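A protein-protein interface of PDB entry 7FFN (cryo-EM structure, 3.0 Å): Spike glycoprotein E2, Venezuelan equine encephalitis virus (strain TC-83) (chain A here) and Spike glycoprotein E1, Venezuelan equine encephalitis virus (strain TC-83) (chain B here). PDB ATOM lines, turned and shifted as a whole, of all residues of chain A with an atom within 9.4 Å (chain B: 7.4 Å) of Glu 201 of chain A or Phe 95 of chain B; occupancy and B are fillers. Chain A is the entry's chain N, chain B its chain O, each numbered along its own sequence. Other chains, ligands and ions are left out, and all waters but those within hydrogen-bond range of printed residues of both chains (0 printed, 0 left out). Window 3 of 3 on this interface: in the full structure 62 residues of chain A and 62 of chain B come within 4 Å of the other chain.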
ATOM      1  N   VAL A 174      -6.199  15.990  24.747  1.00  0.00           N
ATOM      2  CA  VAL A 174      -6.271  16.061  23.297  1.00  0.00           C
ATOM      3  C   VAL A 174      -4.851  16.025  22.746  1.00  0.00           C
ATOM      4  O   VAL A 174      -3.883  16.365  23.435  1.00  0.00           O
ATOM      5  CB  VAL A 174      -7.047  17.319  22.851  1.00  0.00           C
ATOM      6  CG1 VAL A 174      -6.205  18.562  22.968  1.00  0.00           C
ATOM      7  CG2 VAL A 174      -7.614  17.160  21.456  1.00  0.00           C
ATOM      8  N   VAL A 198     -12.222   9.429  19.172  1.00  0.00           N
ATOM      9  CA  VAL A 198     -12.147  10.406  18.096  1.00  0.00           C
ATOM     10  C   VAL A 198     -13.516  11.049  17.944  1.00  0.00           C
ATOM     11  O   VAL A 198     -14.538  10.359  17.985  1.00  0.00           O
ATOM     12  CB  VAL A 198     -11.697   9.745  16.777  1.00  0.00           C
ATOM     13  CG1 VAL A 198     -11.642  10.748  15.634  1.00  0.00           C
ATOM     14  CG2 VAL A 198     -10.350   9.089  16.959  1.00  0.00           C
ATOM     15  N   GLU A 199     -13.540  12.372  17.789  1.00  0.00           N
ATOM     16  CA  GLU A 199     -14.777  13.104  17.553  1.00  0.00           C
ATOM     17  C   GLU A 199     -14.586  14.042  16.373  1.00  0.00           C
ATOM     18  O   GLU A 199     -13.695  14.896  16.400  1.00  0.00           O
ATOM     19  CB  GLU A 199     -15.201  13.884  18.797  1.00  0.00           C
ATOM     20  CG  GLU A 199     -15.634  13.006  19.956  1.00  0.00           C
ATOM     21  CD  GLU A 199     -16.063  13.812  21.155  1.00  0.00           C
ATOM     22  OE1 GLU A 199     -15.884  15.045  21.129  1.00  0.00           O
ATOM     23  OE2 GLU A 199     -16.585  13.219  22.119  1.00  0.00           O
ATOM     24  N   CYS A 200     -15.428  13.892  15.353  1.00  0.00           N
ATOM     25  CA  CYS A 200     -15.359  14.706  14.147  1.00  0.00           C
ATOM     26  C   CYS A 200     -16.741  15.260  13.848  1.00  0.00           C
ATOM     27  O   CYS A 200     -17.752  14.695  14.271  1.00  0.00           O
ATOM     28  CB  CYS A 200     -14.873  13.894  12.949  1.00  0.00           C
ATOM     29  SG  CYS A 200     -13.318  13.026  13.204  1.00  0.00           S
ATOM     30  N   GLU A 201     -16.785  16.381  13.131  1.00  0.00           N
ATOM     31  CA  GLU A 201     -18.054  17.038  12.824  1.00  0.00           C
ATOM     32  C   GLU A 201     -18.056  17.556  11.384  1.00  0.00           C
ATOM     33  O   GLU A 201     -18.305  18.732  11.122  1.00  0.00           O
ATOM     34  CB  GLU A 201     -18.315  18.137  13.855  1.00  0.00           C
ATOM     35  CG  GLU A 201     -19.780  18.533  14.063  1.00  0.00           C
ATOM     36  CD  GLU A 201     -20.208  19.754  13.273  1.00  0.00           C
ATOM     37  OE1 GLU A 201     -19.351  20.630  13.032  1.00  0.00           O
ATOM     38  OE2 GLU A 201     -21.395  19.842  12.907  1.00  0.00           O
ATOM     39  N   CYS A 202     -17.726  16.695  10.419  1.00  0.00           N
ATOM     40  CA  CYS A 202     -17.719  17.168   9.036  1.00  0.00           C
ATOM     41  C   CYS A 202     -19.004  16.838   8.285  1.00  0.00           C
ATOM     42  O   CYS A 202     -19.503  17.667   7.518  1.00  0.00           O
ATOM     43  CB  CYS A 202     -16.531  16.587   8.270  1.00  0.00           C
ATOM     44  SG  CYS A 202     -16.675  14.838   7.894  1.00  0.00           S
ATOM     45  N   GLY A 203     -19.543  15.637   8.480  1.00  0.00           N
ATOM     46  CA  GLY A 203     -20.791  15.251   7.851  1.00  0.00           C
ATOM     47  C   GLY A 203     -21.931  15.333   8.839  1.00  0.00           C
ATOM     48  O   GLY A 203     -22.502  16.404   9.064  1.00  0.00           O
ATOM     49  N   GLY A 204     -22.277  14.194   9.434  1.00  0.00           N
ATOM     50  CA  GLY A 204     -23.191  14.184  10.555  1.00  0.00           C
ATOM     51  C   GLY A 204     -22.441  14.445  11.843  1.00  0.00           C
ATOM     52  O   GLY A 204     -21.713  15.438  11.952  1.00  0.00           O
ATOM     53  N   THR A 205     -22.596  13.568  12.831  1.00  0.00           N
ATOM     54  CA  THR A 205     -21.922  13.713  14.116  1.00  0.00           C
ATOM     55  C   THR A 205     -21.339  12.365  14.501  1.00  0.00           C
ATOM     56  O   THR A 205     -22.065  11.369  14.549  1.00  0.00           O
ATOM     57  CB  THR A 205     -22.883  14.222  15.194  1.00  0.00           C
ATOM     58  OG1 THR A 205     -23.357  15.526  14.833  1.00  0.00           O
ATOM     59  CG2 THR A 205     -22.191  14.304  16.542  1.00  0.00           C
ATOM     60  N   LYS A 206     -20.037  12.327  14.772  1.00  0.00           N
ATOM     61  CA  LYS A 206     -19.328  11.075  15.004  1.00  0.00           C
ATOM     62  C   LYS A 206     -18.604  11.094  16.342  1.00  0.00           C
ATOM     63  O   LYS A 206     -17.778  11.978  16.598  1.00  0.00           O
ATOM     64  CB  LYS A 206     -18.349  10.800  13.866  1.00  0.00           C
ATOM     65  CG  LYS A 206     -17.399   9.660  14.139  1.00  0.00           C
ATOM     66  CD  LYS A 206     -16.700   9.221  12.869  1.00  0.00           C
ATOM     67  CE  LYS A 206     -15.601  10.179  12.456  1.00  0.00           C
ATOM     68  NZ  LYS A 206     -16.080  11.181  11.457  1.00  0.00           N
ATOM     69  N   ILE A 207     -18.921  10.116  17.187  1.00  0.00           N
ATOM     70  CA  ILE A 207     -18.171   9.816  18.400  1.00  0.00           C
ATOM     71  C   ILE A 207     -17.783   8.349  18.330  1.00  0.00           C
ATOM     72  O   ILE A 207     -18.639   7.467  18.462  1.00  0.00           O
ATOM     73  CB  ILE A 207     -18.984  10.104  19.672  1.00  0.00           C
ATOM     74  CG1 ILE A 207     -19.322  11.591  19.777  1.00  0.00           C
ATOM     75  CG2 ILE A 207     -18.215   9.660  20.907  1.00  0.00           C
ATOM     76  CD1 ILE A 207     -20.307  11.913  20.879  1.00  0.00           C
ATOM     77  N   GLN A 219     -14.622  10.072   4.946  1.00  0.00           N
ATOM     78  CA  GLN A 219     -15.091  11.445   4.922  1.00  0.00           C
ATOM     79  C   GLN A 219     -14.147  12.317   5.750  1.00  0.00           C
ATOM     80  O   GLN A 219     -13.072  11.869   6.161  1.00  0.00           O
ATOM     81  CB  GLN A 219     -16.533  11.482   5.416  1.00  0.00           C
ATOM     82  CG  GLN A 219     -16.693  10.877   6.793  1.00  0.00           C
ATOM     83  CD  GLN A 219     -18.141  10.706   7.186  1.00  0.00           C
ATOM     84  OE1 GLN A 219     -19.041  11.137   6.471  1.00  0.00           O
ATOM     85  NE2 GLN A 219     -18.377  10.045   8.311  1.00  0.00           N
ATOM     86  N   CYS A 220     -14.547  13.575   5.983  1.00  0.00           N
ATOM     87  CA  CYS A 220     -13.827  14.565   6.797  1.00  0.00           C
ATOM     88  C   CYS A 220     -12.417  14.818   6.255  1.00  0.00           C
ATOM     89  O   CYS A 220     -11.421  14.468   6.877  1.00  0.00           O
ATOM     90  CB  CYS A 220     -13.760  14.143   8.273  1.00  0.00           C
ATOM     91  SG  CYS A 220     -15.330  13.975   9.135  1.00  0.00           S
ATOM     92  N   THR A 221     -12.353  15.427   5.074  1.00  0.00           N
ATOM     93  CA  THR A 221     -11.071  15.536   4.376  1.00  0.00           C
ATOM     94  C   THR A 221     -10.346  16.839   4.734  1.00  0.00           C
ATOM     95  O   THR A 221      -9.908  17.598   3.869  1.00  0.00           O
ATOM     96  CB  THR A 221     -11.296  15.410   2.871  1.00  0.00           C
ATOM     97  OG1 THR A 221     -12.291  14.411   2.634  1.00  0.00           O
ATOM     98  CG2 THR A 221     -10.027  14.906   2.167  1.00  0.00           C
ATOM     99  N   LYS A 222     -10.223  17.101   6.039  1.00  0.00           N
ATOM    100  CA  LYS A 222      -9.385  18.156   6.603  1.00  0.00           C
ATOM    101  C   LYS A 222      -8.869  17.684   7.957  1.00  0.00           C
ATOM    102  O   LYS A 222      -9.512  16.871   8.625  1.00  0.00           O
ATOM    103  CB  LYS A 222     -10.128  19.488   6.789  1.00  0.00           C
ATOM    104  CG  LYS A 222     -10.378  20.290   5.526  1.00  0.00           C
ATOM    105  CD  LYS A 222     -11.095  21.594   5.806  1.00  0.00           C
ATOM    106  CE  LYS A 222     -11.328  22.354   4.516  1.00  0.00           C
ATOM    107  NZ  LYS A 222     -12.030  23.644   4.739  1.00  0.00           N
ATOM    108  N   LYS A 223      -7.706  18.206   8.360  1.00  0.00           N
ATOM    109  CA  LYS A 223      -7.185  17.879   9.685  1.00  0.00           C
ATOM    110  C   LYS A 223      -8.022  18.501  10.788  1.00  0.00           C
ATOM    111  O   LYS A 223      -8.247  17.868  11.825  1.00  0.00           O
ATOM    112  CB  LYS A 223      -5.737  18.339   9.843  1.00  0.00           C
ATOM    113  CG  LYS A 223      -4.683  17.491   9.166  1.00  0.00           C
ATOM    114  CD  LYS A 223      -3.311  18.030   9.535  1.00  0.00           C
ATOM    115  CE  LYS A 223      -2.176  17.224   8.933  1.00  0.00           C
ATOM    116  NZ  LYS A 223      -0.856  17.812   9.306  1.00  0.00           N
ATOM    117  N   GLU A 224      -8.508  19.722  10.577  1.00  0.00           N
ATOM    118  CA  GLU A 224      -9.213  20.455  11.617  1.00  0.00           C
ATOM    119  C   GLU A 224     -10.625  19.943  11.863  1.00  0.00           C
ATOM    120  O   GLU A 224     -11.258  20.375  12.830  1.00  0.00           O
ATOM    121  CB  GLU A 224      -9.257  21.939  11.262  1.00  0.00           C
ATOM    122  CG  GLU A 224      -7.882  22.581  11.229  1.00  0.00           C
ATOM    123  CD  GLU A 224      -7.930  24.056  10.895  1.00  0.00           C
ATOM    124  OE1 GLU A 224      -9.031  24.562  10.581  1.00  0.00           O
ATOM    125  OE2 GLU A 224      -6.868  24.713  10.943  1.00  0.00           O
ATOM    126  N   GLN A 225     -11.131  19.044  11.018  1.00  0.00           N
ATOM    127  CA  GLN A 225     -12.463  18.492  11.227  1.00  0.00           C
ATOM    128  C   GLN A 225     -12.519  17.529  12.402  1.00  0.00           C
ATOM    129  O   GLN A 225     -13.612  17.248  12.899  1.00  0.00           O
ATOM    130  CB  GLN A 225     -12.946  17.761   9.971  1.00  0.00           C
ATOM    131  CG  GLN A 225     -13.150  18.625   8.741  1.00  0.00           C
ATOM    132  CD  GLN A 225     -14.260  19.639   8.908  1.00  0.00           C
ATOM    133  OE1 GLN A 225     -15.260  19.382   9.575  1.00  0.00           O
ATOM    134  NE2 GLN A 225     -14.097  20.797   8.283  1.00  0.00           N
ATOM    135  N   CYS A 226     -11.380  17.021  12.859  1.00  0.00           N
ATOM    136  CA  CYS A 226     -11.349  15.942  13.832  1.00  0.00           C
ATOM    137  C   CYS A 226     -10.469  16.299  15.017  1.00  0.00           C
ATOM    138  O   CYS A 226      -9.387  16.864  14.853  1.00  0.00           O
ATOM    139  CB  CYS A 226     -10.845  14.653  13.194  1.00  0.00           C
ATOM    140  SG  CYS A 226     -11.995  13.981  12.005  1.00  0.00           S
ATOM    141  N   ARG A 227     -10.942  15.951  16.209  1.00  0.00           N
ATOM    142  CA  ARG A 227     -10.183  16.099  17.440  1.00  0.00           C
ATOM    143  C   ARG A 227      -9.901  14.712  17.989  1.00  0.00           C
ATOM    144  O   ARG A 227     -10.820  13.905  18.149  1.00  0.00           O
ATOM    145  CB  ARG A 227     -10.949  16.935  18.463  1.00  0.00           C
ATOM    146  CG  ARG A 227     -11.236  18.350  18.018  1.00  0.00           C
ATOM    147  CD  ARG A 227      -9.975  19.173  17.935  1.00  0.00           C
ATOM    148  NE  ARG A 227     -10.261  20.567  17.622  1.00  0.00           N
ATOM    149  CZ  ARG A 227     -10.274  21.063  16.391  1.00  0.00           C
ATOM    150  NH1 ARG A 227     -10.005  20.277  15.363  1.00  0.00           N
ATOM    151  NH2 ARG A 227     -10.545  22.339  16.188  1.00  0.00           N
ATOM    152  N   ALA A 228      -8.637  14.430  18.263  1.00  0.00           N
ATOM    153  CA  ALA A 228      -8.209  13.116  18.722  1.00  0.00           C
ATOM    154  C   ALA A 228      -7.770  13.231  20.174  1.00  0.00           C
ATOM    155  O   ALA A 228      -6.779  13.903  20.474  1.00  0.00           O
ATOM    156  CB  ALA A 228      -7.083  12.575  17.847  1.00  0.00           C
ATOM    157  N   TYR A 229      -8.503  12.578  21.069  1.00  0.00           N
ATOM    158  CA  TYR A 229      -8.167  12.586  22.481  1.00  0.00           C
ATOM    159  C   TYR A 229      -7.331  11.353  22.821  1.00  0.00           C
ATOM    160  O   TYR A 229      -7.001  10.545  21.956  1.00  0.00           O
ATOM    161  CB  TYR A 229      -9.433  12.648  23.327  1.00  0.00           C
ATOM    162  CG  TYR A 229     -10.266  13.872  23.053  1.00  0.00           C
ATOM    163  CD1 TYR A 229      -9.887  15.112  23.538  1.00  0.00           C
ATOM    164  CD2 TYR A 229     -11.436  13.787  22.319  1.00  0.00           C
ATOM    165  CE1 TYR A 229     -10.639  16.233  23.285  1.00  0.00           C
ATOM    166  CE2 TYR A 229     -12.198  14.903  22.064  1.00  0.00           C
ATOM    167  CZ  TYR A 229     -11.795  16.123  22.551  1.00  0.00           C
ATOM    168  OH  TYR A 229     -12.550  17.243  22.305  1.00  0.00           O
ATOM    169  N   CYS B  62     -18.050  20.318  24.998  1.00  0.00           N
ATOM    170  CA  CYS B  62     -17.958  20.960  23.694  1.00  0.00           C
ATOM    171  C   CYS B  62     -19.328  20.942  23.021  1.00  0.00           C
ATOM    172  O   CYS B  62     -19.907  19.867  22.827  1.00  0.00           O
ATOM    173  CB  CYS B  62     -16.921  20.258  22.818  1.00  0.00           C
ATOM    174  SG  CYS B  62     -15.214  20.298  23.427  1.00  0.00           S
ATOM    175  N   CYS B  63     -19.815  22.127  22.637  1.00  0.00           N
ATOM    176  CA  CYS B  63     -21.154  22.348  22.075  1.00  0.00           C
ATOM    177  C   CYS B  63     -22.253  21.725  22.937  1.00  0.00           C
ATOM    178  O   CYS B  63     -23.048  20.898  22.491  1.00  0.00           O
ATOM    179  CB  CYS B  63     -21.247  21.864  20.626  1.00  0.00           C
ATOM    180  SG  CYS B  63     -20.749  23.087  19.382  1.00  0.00           S
ATOM    181  N   TYR B  85     -13.062  28.840  24.858  1.00  0.00           N
ATOM    182  CA  TYR B  85     -12.451  28.003  23.825  1.00  0.00           C
ATOM    183  C   TYR B  85     -11.094  27.520  24.314  1.00  0.00           C
ATOM    184  O   TYR B  85     -10.064  28.161  24.074  1.00  0.00           O
ATOM    185  CB  TYR B  85     -12.342  28.762  22.503  1.00  0.00           C
ATOM    186  CG  TYR B  85     -11.851  27.935  21.346  1.00  0.00           C
ATOM    187  CD1 TYR B  85     -12.628  26.914  20.816  1.00  0.00           C
ATOM    188  CD2 TYR B  85     -10.629  28.204  20.749  1.00  0.00           C
ATOM    189  CE1 TYR B  85     -12.185  26.160  19.756  1.00  0.00           C
ATOM    190  CE2 TYR B  85     -10.185  27.462  19.678  1.00  0.00           C
ATOM    191  CZ  TYR B  85     -10.967  26.441  19.189  1.00  0.00           C
ATOM    192  OH  TYR B  85     -10.518  25.700  18.123  1.00  0.00           O
ATOM    193  N   ALA B  92      -6.235  22.349  20.275  1.00  0.00           N
ATOM    194  CA  ALA B  92      -7.487  22.832  20.833  1.00  0.00           C
ATOM    195  C   ALA B  92      -8.266  21.694  21.473  1.00  0.00           C
ATOM    196  O   ALA B  92      -8.131  20.531  21.094  1.00  0.00           O
ATOM    197  CB  ALA B  92      -8.334  23.499  19.754  1.00  0.00           C
ATOM    198  N   TYR B  93      -9.090  22.038  22.456  1.00  0.00           N
ATOM    199  CA  TYR B  93      -9.857  21.021  23.156  1.00  0.00           C
ATOM    200  C   TYR B  93     -11.229  20.800  22.539  1.00  0.00           C
ATOM    201  O   TYR B  93     -11.753  19.684  22.596  1.00  0.00           O
ATOM    202  CB  TYR B  93     -10.006  21.388  24.635  1.00  0.00           C
ATOM    203  CG  TYR B  93     -10.652  20.318  25.483  1.00  0.00           C
ATOM    204  CD1 TYR B  93      -9.927  19.218  25.918  1.00  0.00           C
ATOM    205  CD2 TYR B  93     -11.988  20.409  25.849  1.00  0.00           C
ATOM    206  CE1 TYR B  93     -10.514  18.241  26.699  1.00  0.00           C
ATOM    207  CE2 TYR B  93     -12.584  19.438  26.623  1.00  0.00           C
ATOM    208  CZ  TYR B  93     -11.843  18.358  27.044  1.00  0.00           C
ATOM    209  OH  TYR B  93     -12.443  17.393  27.817  1.00  0.00           O
ATOM    210  N   CYS B  94     -11.825  21.832  21.955  1.00  0.00           N
ATOM    211  CA  CYS B  94     -13.095  21.716  21.260  1.00  0.00           C
ATOM    212  C   CYS B  94     -12.896  21.978  19.771  1.00  0.00           C
ATOM    213  O   CYS B  94     -11.815  22.359  19.316  1.00  0.00           O
ATOM    214  CB  CYS B  94     -14.129  22.678  21.851  1.00  0.00           C
ATOM    215  SG  CYS B  94     -14.705  22.266  23.515  1.00  0.00           S
ATOM    216  N   PHE B  95     -13.960  21.754  19.004  1.00  0.00           N
ATOM    217  CA  PHE B  95     -13.995  22.116  17.597  1.00  0.00           C
ATOM    218  C   PHE B  95     -14.983  23.228  17.285  1.00  0.00           C
ATOM    219  O   PHE B  95     -14.892  23.823  16.207  1.00  0.00           O
ATOM    220  CB  PHE B  95     -14.312  20.888  16.721  1.00  0.00           C
ATOM    221  CG  PHE B  95     -15.573  20.151  17.112  1.00  0.00           C
ATOM    222  CD1 PHE B  95     -15.515  19.079  17.989  1.00  0.00           C
ATOM    223  CD2 PHE B  95     -16.806  20.516  16.592  1.00  0.00           C
ATOM    224  CE1 PHE B  95     -16.662  18.399  18.350  1.00  0.00           C
ATOM    225  CE2 PHE B  95     -17.956  19.844  16.959  1.00  0.00           C
ATOM    226  CZ  PHE B  95     -17.883  18.783  17.834  1.00  0.00           C
ATOM    227  N   CYS B  96     -15.911  23.522  18.188  1.00  0.00           N
ATOM    228  CA  CYS B  96     -16.912  24.551  17.980  1.00  0.00           C
ATOM    229  C   CYS B  96     -16.290  25.932  18.149  1.00  0.00           C
ATOM    230  O   CYS B  96     -15.191  26.084  18.683  1.00  0.00           O
ATOM    231  CB  CYS B  96     -18.055  24.372  18.974  1.00  0.00           C
ATOM    232  SG  CYS B  96     -18.799  22.725  18.963  1.00  0.00           S
ATOM    233  N   ASP B  97     -17.010  26.951  17.689  1.00  0.00           N
ATOM    234  CA  ASP B  97     -16.557  28.324  17.881  1.00  0.00           C
ATOM    235  C   ASP B  97     -17.197  28.956  19.110  1.00  0.00           C
ATOM    236  O   ASP B  97     -16.514  29.593  19.916  1.00  0.00           O
ATOM    237  CB  ASP B  97     -16.854  29.161  16.637  1.00  0.00           C
ATOM    238  CG  ASP B  97     -15.996  28.768  15.453  1.00  0.00           C
ATOM    239  OD1 ASP B  97     -14.870  28.274  15.670  1.00  0.00           O
ATOM    240  OD2 ASP B  97     -16.446  28.957  14.304  1.00  0.00           O
ATOM    241  N   THR B  98     -18.504  28.801  19.253  1.00  0.00           N
ATOM    242  CA  THR B  98     -19.255  29.213  20.427  1.00  0.00           C
ATOM    243  C   THR B  98     -19.929  27.977  21.015  1.00  0.00           C
ATOM    244  O   THR B  98     -19.597  26.844  20.654  1.00  0.00           O
ATOM    245  CB  THR B  98     -20.274  30.300  20.086  1.00  0.00           C
ATOM    246  OG1 THR B  98     -21.187  29.812  19.096  1.00  0.00           O
ATOM    247  CG2 THR B  98     -19.574  31.548  19.567  1.00  0.00           C
ATOM    248  N   ASN B 100     -19.655  26.524  23.815  1.00  0.00           N
ATOM    249  CA  ASN B 100     -18.890  25.697  24.735  1.00  0.00           C
ATOM    250  C   ASN B 100     -19.066  26.218  26.153  1.00  0.00           C
ATOM    251  O   ASN B 100     -19.256  27.416  26.374  1.00  0.00           O
ATOM    252  CB  ASN B 100     -17.412  25.698  24.380  1.00  0.00           C
ATOM    253  CG  ASN B 100     -17.138  25.094  23.039  1.00  0.00           C
ATOM    254  OD1 ASN B 100     -17.740  24.096  22.664  1.00  0.00           O
ATOM    255  ND2 ASN B 100     -16.216  25.696  22.301  1.00  0.00           N
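O of Cys 94 of chain B sits at hydrogen-bond distance from NE of Arg 227 of chain A, 2.9 Å away.
The side-chain hydroxyl of Tyr 229 of chain A sits at hydrogen-bond distance from the backbone carbonyl oxygen of Tyr 93 of chain B (2.6 Å).
The backbone NH (N) of Arg 227 of chain A is in hydrogen-bond range of the backbone carbonyl oxygen (O) of Glu 199 of chain A.
The backbone NH (N) of Glu 201 of chain A lies within hydrogen-bond range of the backbone carbonyl oxygen (O) of Gln 225 of chain A (3.3 Å).
The side-chain sulfur (SG) of Cys 94 of chain B lies close to the side-chain amide oxygen (OD1) of Asn 100 of chain B (3.6 Å).
The side-chain sulfur (SG) of Cys 226 of chain A is disulfide-bonded to the side-chain sulfur (SG) of Cys 200 of chain A, 2.0 Å away.
SG of Cys 202 of chain A is disulfide-bonded to SG of Cys 220 of chain A, 2.0 Å away.
SG of Cys 63 of chain B forms a disulfide with SG of Cys 96 of chain B (2.0 Å).
Val 174 of chain A touches Ala 92 of chain B.
Phe 95 of chain B touches Glu 201 of chain A (CE2 to CB, 3.6 Å).
Tyr 85 of chain B touches Arg 227 of chain A (OH to NH2, 3.9 Å).
Arg 227 of chain A touches Ala 92 of chain B (CD to O, 3.9 Å).
Arg 227 of chain A touches Phe 95 of chain B (NH2 to CA, 3.7 Å).
Of the printed residues of chain B, Val 174 of chain A touches Ala 92.
Cys 63 of chain B touches none of the printed residues of chain A.
Of the printed residues of chain A, Ala 92 of chain B touches Val 174 and Arg 227.
Of the printed residues of chain A, Phe 95 of chain B touches Glu 201 and Arg 227.
No residue of chain A comes within 4 Å of Cys 96 of chain B.
The nearest residue of chain B that does not touch Glu 201 of chain A is Cys 96 of chain B (6.3 Å).
The nearest printed residue of chain B that does not touch Arg 227 of chain A is Tyr 93 of chain B (4.8 Å).
Of the 22 printed residues of chain A, 4 touch a printed residue of chain B.
Hydrophobic or aromatic side chains of chain B within 4 Å of the printed part of chain A: Tyr 85, Tyr 93 and Phe 95.
Among the printed residues, 7 pairs touch across the chains.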
